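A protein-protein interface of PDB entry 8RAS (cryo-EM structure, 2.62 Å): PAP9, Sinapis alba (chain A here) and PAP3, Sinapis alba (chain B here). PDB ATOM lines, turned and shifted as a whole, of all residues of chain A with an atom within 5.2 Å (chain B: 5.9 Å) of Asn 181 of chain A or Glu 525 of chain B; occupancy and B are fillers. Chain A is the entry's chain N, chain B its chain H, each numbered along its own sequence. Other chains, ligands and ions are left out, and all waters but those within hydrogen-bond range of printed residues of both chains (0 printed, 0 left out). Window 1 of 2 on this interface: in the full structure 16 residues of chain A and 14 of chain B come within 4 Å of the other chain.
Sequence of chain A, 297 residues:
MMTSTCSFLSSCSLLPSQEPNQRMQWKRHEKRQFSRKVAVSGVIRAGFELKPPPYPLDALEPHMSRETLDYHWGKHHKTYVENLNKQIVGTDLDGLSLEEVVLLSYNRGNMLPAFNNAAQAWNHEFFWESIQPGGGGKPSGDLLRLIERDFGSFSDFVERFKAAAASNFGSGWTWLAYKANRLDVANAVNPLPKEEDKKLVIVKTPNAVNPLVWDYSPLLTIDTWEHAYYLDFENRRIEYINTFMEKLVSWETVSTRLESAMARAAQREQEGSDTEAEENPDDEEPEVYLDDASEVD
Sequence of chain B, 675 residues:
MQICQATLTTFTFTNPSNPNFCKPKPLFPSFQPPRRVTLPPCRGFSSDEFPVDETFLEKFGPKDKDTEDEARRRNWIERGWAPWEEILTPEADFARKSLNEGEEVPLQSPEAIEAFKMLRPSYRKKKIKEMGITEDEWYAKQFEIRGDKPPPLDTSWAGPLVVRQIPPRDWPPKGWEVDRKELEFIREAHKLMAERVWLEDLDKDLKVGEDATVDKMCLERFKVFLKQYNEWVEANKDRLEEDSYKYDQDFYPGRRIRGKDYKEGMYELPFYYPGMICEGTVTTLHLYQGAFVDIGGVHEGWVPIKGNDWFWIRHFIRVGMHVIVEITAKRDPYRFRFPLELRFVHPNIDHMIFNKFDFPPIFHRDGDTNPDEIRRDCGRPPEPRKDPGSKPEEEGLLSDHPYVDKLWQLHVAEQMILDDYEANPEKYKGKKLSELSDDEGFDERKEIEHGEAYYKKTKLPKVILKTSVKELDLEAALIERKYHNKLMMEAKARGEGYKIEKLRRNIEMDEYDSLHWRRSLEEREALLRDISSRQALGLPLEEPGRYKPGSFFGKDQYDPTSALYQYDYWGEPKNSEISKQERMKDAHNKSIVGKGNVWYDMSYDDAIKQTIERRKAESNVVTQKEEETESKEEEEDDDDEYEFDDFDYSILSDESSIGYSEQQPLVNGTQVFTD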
ATOM      1  N   LYS A 179      13.564   4.437  10.786  1.00  0.00           N
ATOM      2  CA  LYS A 179      12.977   3.493   9.834  1.00  0.00           C
ATOM      3  C   LYS A 179      14.035   3.067   8.816  1.00  0.00           C
ATOM      4  O   LYS A 179      14.115   3.574   7.696  1.00  0.00           O
ATOM      5  CB  LYS A 179      11.762   4.110   9.153  1.00  0.00           C
ATOM      6  CG  LYS A 179      10.777   3.097   8.595  1.00  0.00           C
ATOM      7  CD  LYS A 179       9.545   3.781   8.027  1.00  0.00           C
ATOM      8  CE  LYS A 179       8.539   2.766   7.514  1.00  0.00           C
ATOM      9  NZ  LYS A 179       9.141   1.849   6.508  1.00  0.00           N
ATOM     10  N   ALA A 180      14.853   2.098   9.220  1.00  0.00           N
ATOM     11  CA  ALA A 180      15.867   1.536   8.336  1.00  0.00           C
ATOM     12  C   ALA A 180      15.633   0.044   8.147  1.00  0.00           C
ATOM     13  O   ALA A 180      16.570  -0.756   8.238  1.00  0.00           O
ATOM     14  CB  ALA A 180      17.271   1.792   8.889  1.00  0.00           C
ATOM     15  N   ASN A 181      14.388  -0.338   7.887  1.00  0.00           N
ATOM     16  CA  ASN A 181      13.999  -1.739   7.858  1.00  0.00           C
ATOM     17  C   ASN A 181      14.031  -2.304   6.444  1.00  0.00           C
ATOM     18  O   ASN A 181      13.790  -1.600   5.460  1.00  0.00           O
ATOM     19  CB  ASN A 181      12.599  -1.916   8.446  1.00  0.00           C
ATOM     20  CG  ASN A 181      11.513  -1.377   7.537  1.00  0.00           C
ATOM     21  OD1 ASN A 181      11.615  -0.264   7.021  1.00  0.00           O
ATOM     22  ND2 ASN A 181      10.466  -2.167   7.336  1.00  0.00           N
ATOM     23  N   ARG A 182      14.339  -3.598   6.358  1.00  0.00           N
ATOM     24  CA  ARG A 182      14.262  -4.357   5.119  1.00  0.00           C
ATOM     25  C   ARG A 182      13.540  -5.663   5.406  1.00  0.00           C
ATOM     26  O   ARG A 182      13.840  -6.335   6.399  1.00  0.00           O
ATOM     27  CB  ARG A 182      15.655  -4.628   4.540  1.00  0.00           C
ATOM     28  CG  ARG A 182      15.670  -5.620   3.386  1.00  0.00           C
ATOM     29  CD  ARG A 182      14.902  -5.082   2.188  1.00  0.00           C
ATOM     30  NE  ARG A 182      15.581  -3.955   1.561  1.00  0.00           N
ATOM     31  CZ  ARG A 182      14.976  -2.845   1.164  1.00  0.00           C
ATOM     32  NH1 ARG A 182      13.675  -2.671   1.326  1.00  0.00           N
ATOM     33  NH2 ARG A 182      15.694  -1.882   0.592  1.00  0.00           N
ATOM     34  N   LEU A 183      12.597  -6.019   4.543  1.00  0.00           N
ATOM     35  CA  LEU A 183      11.762  -7.191   4.754  1.00  0.00           C
ATOM     36  C   LEU A 183      12.420  -8.437   4.167  1.00  0.00           C
ATOM     37  O   LEU A 183      13.279  -8.362   3.285  1.00  0.00           O
ATOM     38  CB  LEU A 183      10.379  -6.984   4.133  1.00  0.00           C
ATOM     39  CG  LEU A 183       9.366  -6.146   4.920  1.00  0.00           C
ATOM     40  CD1 LEU A 183       9.245  -6.647   6.354  1.00  0.00           C
ATOM     41  CD2 LEU A 183       9.709  -4.660   4.889  1.00  0.00           C
ATOM     42  N   TRP A 214      11.356  -5.829  13.711  1.00  0.00           N
ATOM     43  CA  TRP A 214      10.947  -5.312  12.413  1.00  0.00           C
ATOM     44  C   TRP A 214      12.108  -4.691  11.647  1.00  0.00           C
ATOM     45  O   TRP A 214      11.873  -3.890  10.736  1.00  0.00           O
ATOM     46  CB  TRP A 214       9.829  -4.277  12.570  1.00  0.00           C
ATOM     47  CG  TRP A 214       8.838  -4.577  13.646  1.00  0.00           C
ATOM     48  CD1 TRP A 214       8.311  -5.794  13.962  1.00  0.00           C
ATOM     49  CD2 TRP A 214       8.247  -3.636  14.550  1.00  0.00           C
ATOM     50  NE1 TRP A 214       7.432  -5.671  15.009  1.00  0.00           N
ATOM     51  CE2 TRP A 214       7.374  -4.355  15.388  1.00  0.00           C
ATOM     52  CE3 TRP A 214       8.373  -2.255  14.732  1.00  0.00           C
ATOM     53  CZ2 TRP A 214       6.630  -3.741  16.393  1.00  0.00           C
ATOM     54  CZ3 TRP A 214       7.635  -1.648  15.729  1.00  0.00           C
ATOM     55  CH2 TRP A 214       6.774  -2.390  16.547  1.00  0.00           C
ATOM     56  N   ASP A 215      13.348  -5.033  12.009  1.00  0.00           N
ATOM     57  CA  ASP A 215      14.552  -4.450  11.412  1.00  0.00           C
ATOM     58  C   ASP A 215      14.616  -2.939  11.628  1.00  0.00           C
ATOM     59  O   ASP A 215      15.172  -2.206  10.807  1.00  0.00           O
ATOM     60  CB  ASP A 215      14.659  -4.785   9.921  1.00  0.00           C
ATOM     61  CG  ASP A 215      16.090  -4.767   9.421  1.00  0.00           C
ATOM     62  OD1 ASP A 215      16.970  -5.322  10.110  1.00  0.00           O
ATOM     63  OD2 ASP A 215      16.333  -4.197   8.336  1.00  0.00           O
ATOM     64  N   TYR A 216      14.056  -2.463  12.736  1.00  0.00           N
ATOM     65  CA  TYR A 216      14.098  -1.050  13.074  1.00  0.00           C
ATOM     66  C   TYR A 216      15.333  -0.741  13.917  1.00  0.00           C
ATOM     67  O   TYR A 216      16.030  -1.634  14.404  1.00  0.00           O
ATOM     68  CB  TYR A 216      12.830  -0.635  13.820  1.00  0.00           C
ATOM     69  CG  TYR A 216      11.676  -0.235  12.927  1.00  0.00           C
ATOM     70  CD1 TYR A 216      11.506  -0.808  11.675  1.00  0.00           C
ATOM     71  CD2 TYR A 216      10.753   0.717  13.341  1.00  0.00           C
ATOM     72  CE1 TYR A 216      10.451  -0.445  10.859  1.00  0.00           C
ATOM     73  CE2 TYR A 216       9.695   1.088  12.532  1.00  0.00           C
ATOM     74  CZ  TYR A 216       9.549   0.504  11.292  1.00  0.00           C
ATOM     75  OH  TYR A 216       8.497   0.869  10.484  1.00  0.00           O
ATOM     76  N   ARG A 268      24.550  -0.123   4.719  1.00  0.00           N
ATOM     77  CA  ARG A 268      23.656  -0.973   3.943  1.00  0.00           C
ATOM     78  C   ARG A 268      23.391  -0.418   2.551  1.00  0.00           C
ATOM     79  O   ARG A 268      22.958  -1.171   1.671  1.00  0.00           O
ATOM     80  CB  ARG A 268      22.333  -1.163   4.686  1.00  0.00           C
ATOM     81  CG  ARG A 268      22.412  -2.127   5.857  1.00  0.00           C
ATOM     82  CD  ARG A 268      21.038  -2.392   6.446  1.00  0.00           C
ATOM     83  NE  ARG A 268      20.085  -2.819   5.428  1.00  0.00           N
ATOM     84  CZ  ARG A 268      19.017  -2.123   5.063  1.00  0.00           C
ATOM     85  NH1 ARG A 268      18.725  -0.960   5.624  1.00  0.00           N
ATOM     86  NH2 ARG A 268      18.223  -2.604   4.111  1.00  0.00           N
ATOM     87  N   SER B 520       1.844  -1.657  -0.807  1.00  0.00           N
ATOM     88  CA  SER B 520       2.258  -2.964  -0.319  1.00  0.00           C
ATOM     89  C   SER B 520       3.226  -2.848   0.853  1.00  0.00           C
ATOM     90  O   SER B 520       3.090  -3.566   1.849  1.00  0.00           O
ATOM     91  CB  SER B 520       2.895  -3.754  -1.459  1.00  0.00           C
ATOM     92  OG  SER B 520       1.929  -4.100  -2.434  1.00  0.00           O
ATOM     93  N   LEU B 521       4.228  -1.963   0.754  1.00  0.00           N
ATOM     94  CA  LEU B 521       5.220  -1.931   1.830  1.00  0.00           C
ATOM     95  C   LEU B 521       4.593  -1.456   3.133  1.00  0.00           C
ATOM     96  O   LEU B 521       4.848  -2.031   4.196  1.00  0.00           O
ATOM     97  CB  LEU B 521       6.429  -1.039   1.525  1.00  0.00           C
ATOM     98  CG  LEU B 521       6.354   0.447   1.200  1.00  0.00           C
ATOM     99  CD1 LEU B 521       6.827   1.225   2.408  1.00  0.00           C
ATOM    100  CD2 LEU B 521       7.302   0.744   0.090  1.00  0.00           C
ATOM    101  N   GLU B 522       3.793  -0.384   3.081  1.00  0.00           N
ATOM    102  CA  GLU B 522       3.224   0.131   4.322  1.00  0.00           C
ATOM    103  C   GLU B 522       2.242  -0.861   4.930  1.00  0.00           C
ATOM    104  O   GLU B 522       2.225  -1.057   6.158  1.00  0.00           O
ATOM    105  CB  GLU B 522       2.569   1.495   4.096  1.00  0.00           C
ATOM    106  CG  GLU B 522       1.500   1.541   3.029  1.00  0.00           C
ATOM    107  CD  GLU B 522       1.584   2.803   2.194  1.00  0.00           C
ATOM    108  OE1 GLU B 522       2.599   3.523   2.306  1.00  0.00           O
ATOM    109  OE2 GLU B 522       0.644   3.074   1.420  1.00  0.00           O
ATOM    110  N   GLU B 523       1.436  -1.524   4.092  1.00  0.00           N
ATOM    111  CA  GLU B 523       0.548  -2.551   4.619  1.00  0.00           C
ATOM    112  C   GLU B 523       1.346  -3.695   5.232  1.00  0.00           C
ATOM    113  O   GLU B 523       0.975  -4.222   6.285  1.00  0.00           O
ATOM    114  CB  GLU B 523      -0.387  -3.060   3.523  1.00  0.00           C
ATOM    115  CG  GLU B 523      -1.360  -4.126   4.006  1.00  0.00           C
ATOM    116  CD  GLU B 523      -2.586  -4.250   3.125  1.00  0.00           C
ATOM    117  OE1 GLU B 523      -3.072  -3.215   2.626  1.00  0.00           O
ATOM    118  OE2 GLU B 523      -3.080  -5.382   2.949  1.00  0.00           O
ATOM    119  N   ARG B 524       2.466  -4.069   4.607  1.00  0.00           N
ATOM    120  CA  ARG B 524       3.293  -5.149   5.141  1.00  0.00           C
ATOM    121  C   ARG B 524       3.922  -4.773   6.476  1.00  0.00           C
ATOM    122  O   ARG B 524       4.011  -5.609   7.380  1.00  0.00           O
ATOM    123  CB  ARG B 524       4.379  -5.522   4.131  1.00  0.00           C
ATOM    124  CG  ARG B 524       5.117  -6.806   4.461  1.00  0.00           C
ATOM    125  CD  ARG B 524       4.176  -7.995   4.440  1.00  0.00           C
ATOM    126  NE  ARG B 524       3.367  -8.022   3.226  1.00  0.00           N
ATOM    127  CZ  ARG B 524       3.503  -8.914   2.256  1.00  0.00           C
ATOM    128  NH1 ARG B 524       4.407  -9.877   2.322  1.00  0.00           N
ATOM    129  NH2 ARG B 524       2.711  -8.838   1.189  1.00  0.00           N
ATOM    130  N   GLU B 525       4.392  -3.532   6.615  1.00  0.00           N
ATOM    131  CA  GLU B 525       4.995  -3.123   7.883  1.00  0.00           C
ATOM    132  C   GLU B 525       3.958  -3.082   8.997  1.00  0.00           C
ATOM    133  O   GLU B 525       4.210  -3.567  10.111  1.00  0.00           O
ATOM    134  CB  GLU B 525       5.687  -1.766   7.742  1.00  0.00           C
ATOM    135  CG  GLU B 525       7.094  -1.846   7.168  1.00  0.00           C
ATOM    136  CD  GLU B 525       7.190  -1.310   5.756  1.00  0.00           C
ATOM    137  OE1 GLU B 525       6.601  -0.244   5.482  1.00  0.00           O
ATOM    138  OE2 GLU B 525       7.845  -1.962   4.916  1.00  0.00           O
ATOM    139  N   ALA B 526       2.782  -2.512   8.715  1.00  0.00           N
ATOM    140  CA  ALA B 526       1.696  -2.581   9.685  1.00  0.00           C
ATOM    141  C   ALA B 526       1.366  -4.031  10.017  1.00  0.00           C
ATOM    142  O   ALA B 526       1.066  -4.364  11.169  1.00  0.00           O
ATOM    143  CB  ALA B 526       0.467  -1.850   9.149  1.00  0.00           C
ATOM    144  N   LEU B 527       1.457  -4.913   9.020  1.00  0.00           N
ATOM    145  CA  LEU B 527       1.167  -6.324   9.226  1.00  0.00           C
ATOM    146  C   LEU B 527       2.160  -6.963  10.188  1.00  0.00           C
ATOM    147  O   LEU B 527       1.761  -7.648  11.135  1.00  0.00           O
ATOM    148  CB  LEU B 527       1.178  -7.032   7.872  1.00  0.00           C
ATOM    149  CG  LEU B 527       0.459  -8.359   7.672  1.00  0.00           C
ATOM    150  CD1 LEU B 527      -0.319  -8.259   6.392  1.00  0.00           C
ATOM    151  CD2 LEU B 527       1.443  -9.494   7.567  1.00  0.00           C
ATOM    152  N   LEU B 528       3.458  -6.741   9.967  1.00  0.00           N
ATOM    153  CA  LEU B 528       4.473  -7.298  10.859  1.00  0.00           C
ATOM    154  C   LEU B 528       4.324  -6.757  12.275  1.00  0.00           C
ATOM    155  O   LEU B 528       4.498  -7.499  13.251  1.00  0.00           O
ATOM    156  CB  LEU B 528       5.881  -7.023  10.325  1.00  0.00           C
ATOM    157  CG  LEU B 528       6.501  -7.960   9.281  1.00  0.00           C
ATOM    158  CD1 LEU B 528       6.750  -9.321   9.911  1.00  0.00           C
ATOM    159  CD2 LEU B 528       5.657  -8.106   8.028  1.00  0.00           C
ATOM    160  N   ARG B 529       4.007  -5.467  12.411  1.00  0.00           N
ATOM    161  CA  ARG B 529       3.720  -4.949  13.745  1.00  0.00           C
ATOM    162  C   ARG B 529       2.513  -5.649  14.361  1.00  0.00           C
ATOM    163  O   ARG B 529       2.490  -5.901  15.574  1.00  0.00           O
ATOM    164  CB  ARG B 529       3.502  -3.437  13.695  1.00  0.00           C
ATOM    165  CG  ARG B 529       4.703  -2.660  13.185  1.00  0.00           C
ATOM    166  CD  ARG B 529       4.607  -1.183  13.537  1.00  0.00           C
ATOM    167  NE  ARG B 529       3.907  -0.407  12.521  1.00  0.00           N
ATOM    168  CZ  ARG B 529       2.839   0.343  12.757  1.00  0.00           C
ATOM    169  NH1 ARG B 529       2.322   0.446  13.971  1.00  0.00           N
ATOM    170  NH2 ARG B 529       2.280   1.013  11.753  1.00  0.00           N
ATOM    171  N   ASP B 530       1.512  -5.979  13.541  1.00  0.00           N
ATOM    172  CA  ASP B 530       0.350  -6.711  14.035  1.00  0.00           C
ATOM    173  C   ASP B 530       0.739  -8.098  14.537  1.00  0.00           C
ATOM    174  O   ASP B 530       0.276  -8.533  15.596  1.00  0.00           O
ATOM    175  CB  ASP B 530      -0.709  -6.816  12.937  1.00  0.00           C
ATOM    176  CG  ASP B 530      -1.656  -5.636  12.928  1.00  0.00           C
ATOM    177  OD1 ASP B 530      -2.336  -5.406  13.950  1.00  0.00           O
ATOM    178  OD2 ASP B 530      -1.720  -4.940  11.895  1.00  0.00           O
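NZ of Lys 179 of chain A is in salt-bridge range of OE1 of Glu 525 of chain B, 3.4 Å away.
The side-chain amino group (NZ) of Lys 179 of chain A sits at hydrogen-bond distance from the side-chain amide oxygen (OD1) of Asn 181 of chain A (3.3 Å).
ND2 of Asn 181 of chain A touches CG of Glu 525 of chain B (3.4 Å).
Leu 183 of chain A touches Glu 525 of chain B (CD2 to OE2, 3.3 Å).
Trp 214 of chain A touches Leu 528 of chain B.
CD of Arg 529 of chain B touches CZ3 of Trp 214 of chain A, at 3.8 Å.
Asn 181 of chain A touches just one residue of chain B: Glu 525.
Of the printed residues of chain B, Leu 183 of chain A touches Glu 525 (3.3 Å).
Of the printed residues of chain B, Trp 214 of chain A touches Leu 528 (3.9 Å) and Arg 529 (3.8 Å).
Tyr 216 of chain A touches none of the printed residues of chain B.
Leu 521 of chain B touches none of the printed residues of chain A.
Of chain A, only Lys 179, Asn 181 and Leu 183 come within 4 Å of Glu 525 of chain B.
Of the printed residues of chain A, Arg 529 of chain B touches Trp 214 (3.8 Å).
The nearest residue of chain A that does not touch Glu 525 of chain B is Tyr 216 of chain A (4.5 Å).
Of the 11 printed residues of chain B, 3 touch a printed residue of chain A.
Of the 9 printed residues of chain A, 4 touch a printed residue of chain B.
Printed residues of chain A that touch a printed residue of chain B: Lys 179, Asn 181, Leu 183 and Trp 214.
Hydrophobic or aromatic side chains of chain A within 4 Å of the printed part of chain B: Leu 183 and Trp 214.
Among the printed residues, 5 pairs touch across the chains.
Among the printed residues, Asp or Glu carboxylates within 4 Å of a Lys or Arg side-chain nitrogen of the other chain: Lys 179 of chain A with Glu 525 of chain B (3.4 Å).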
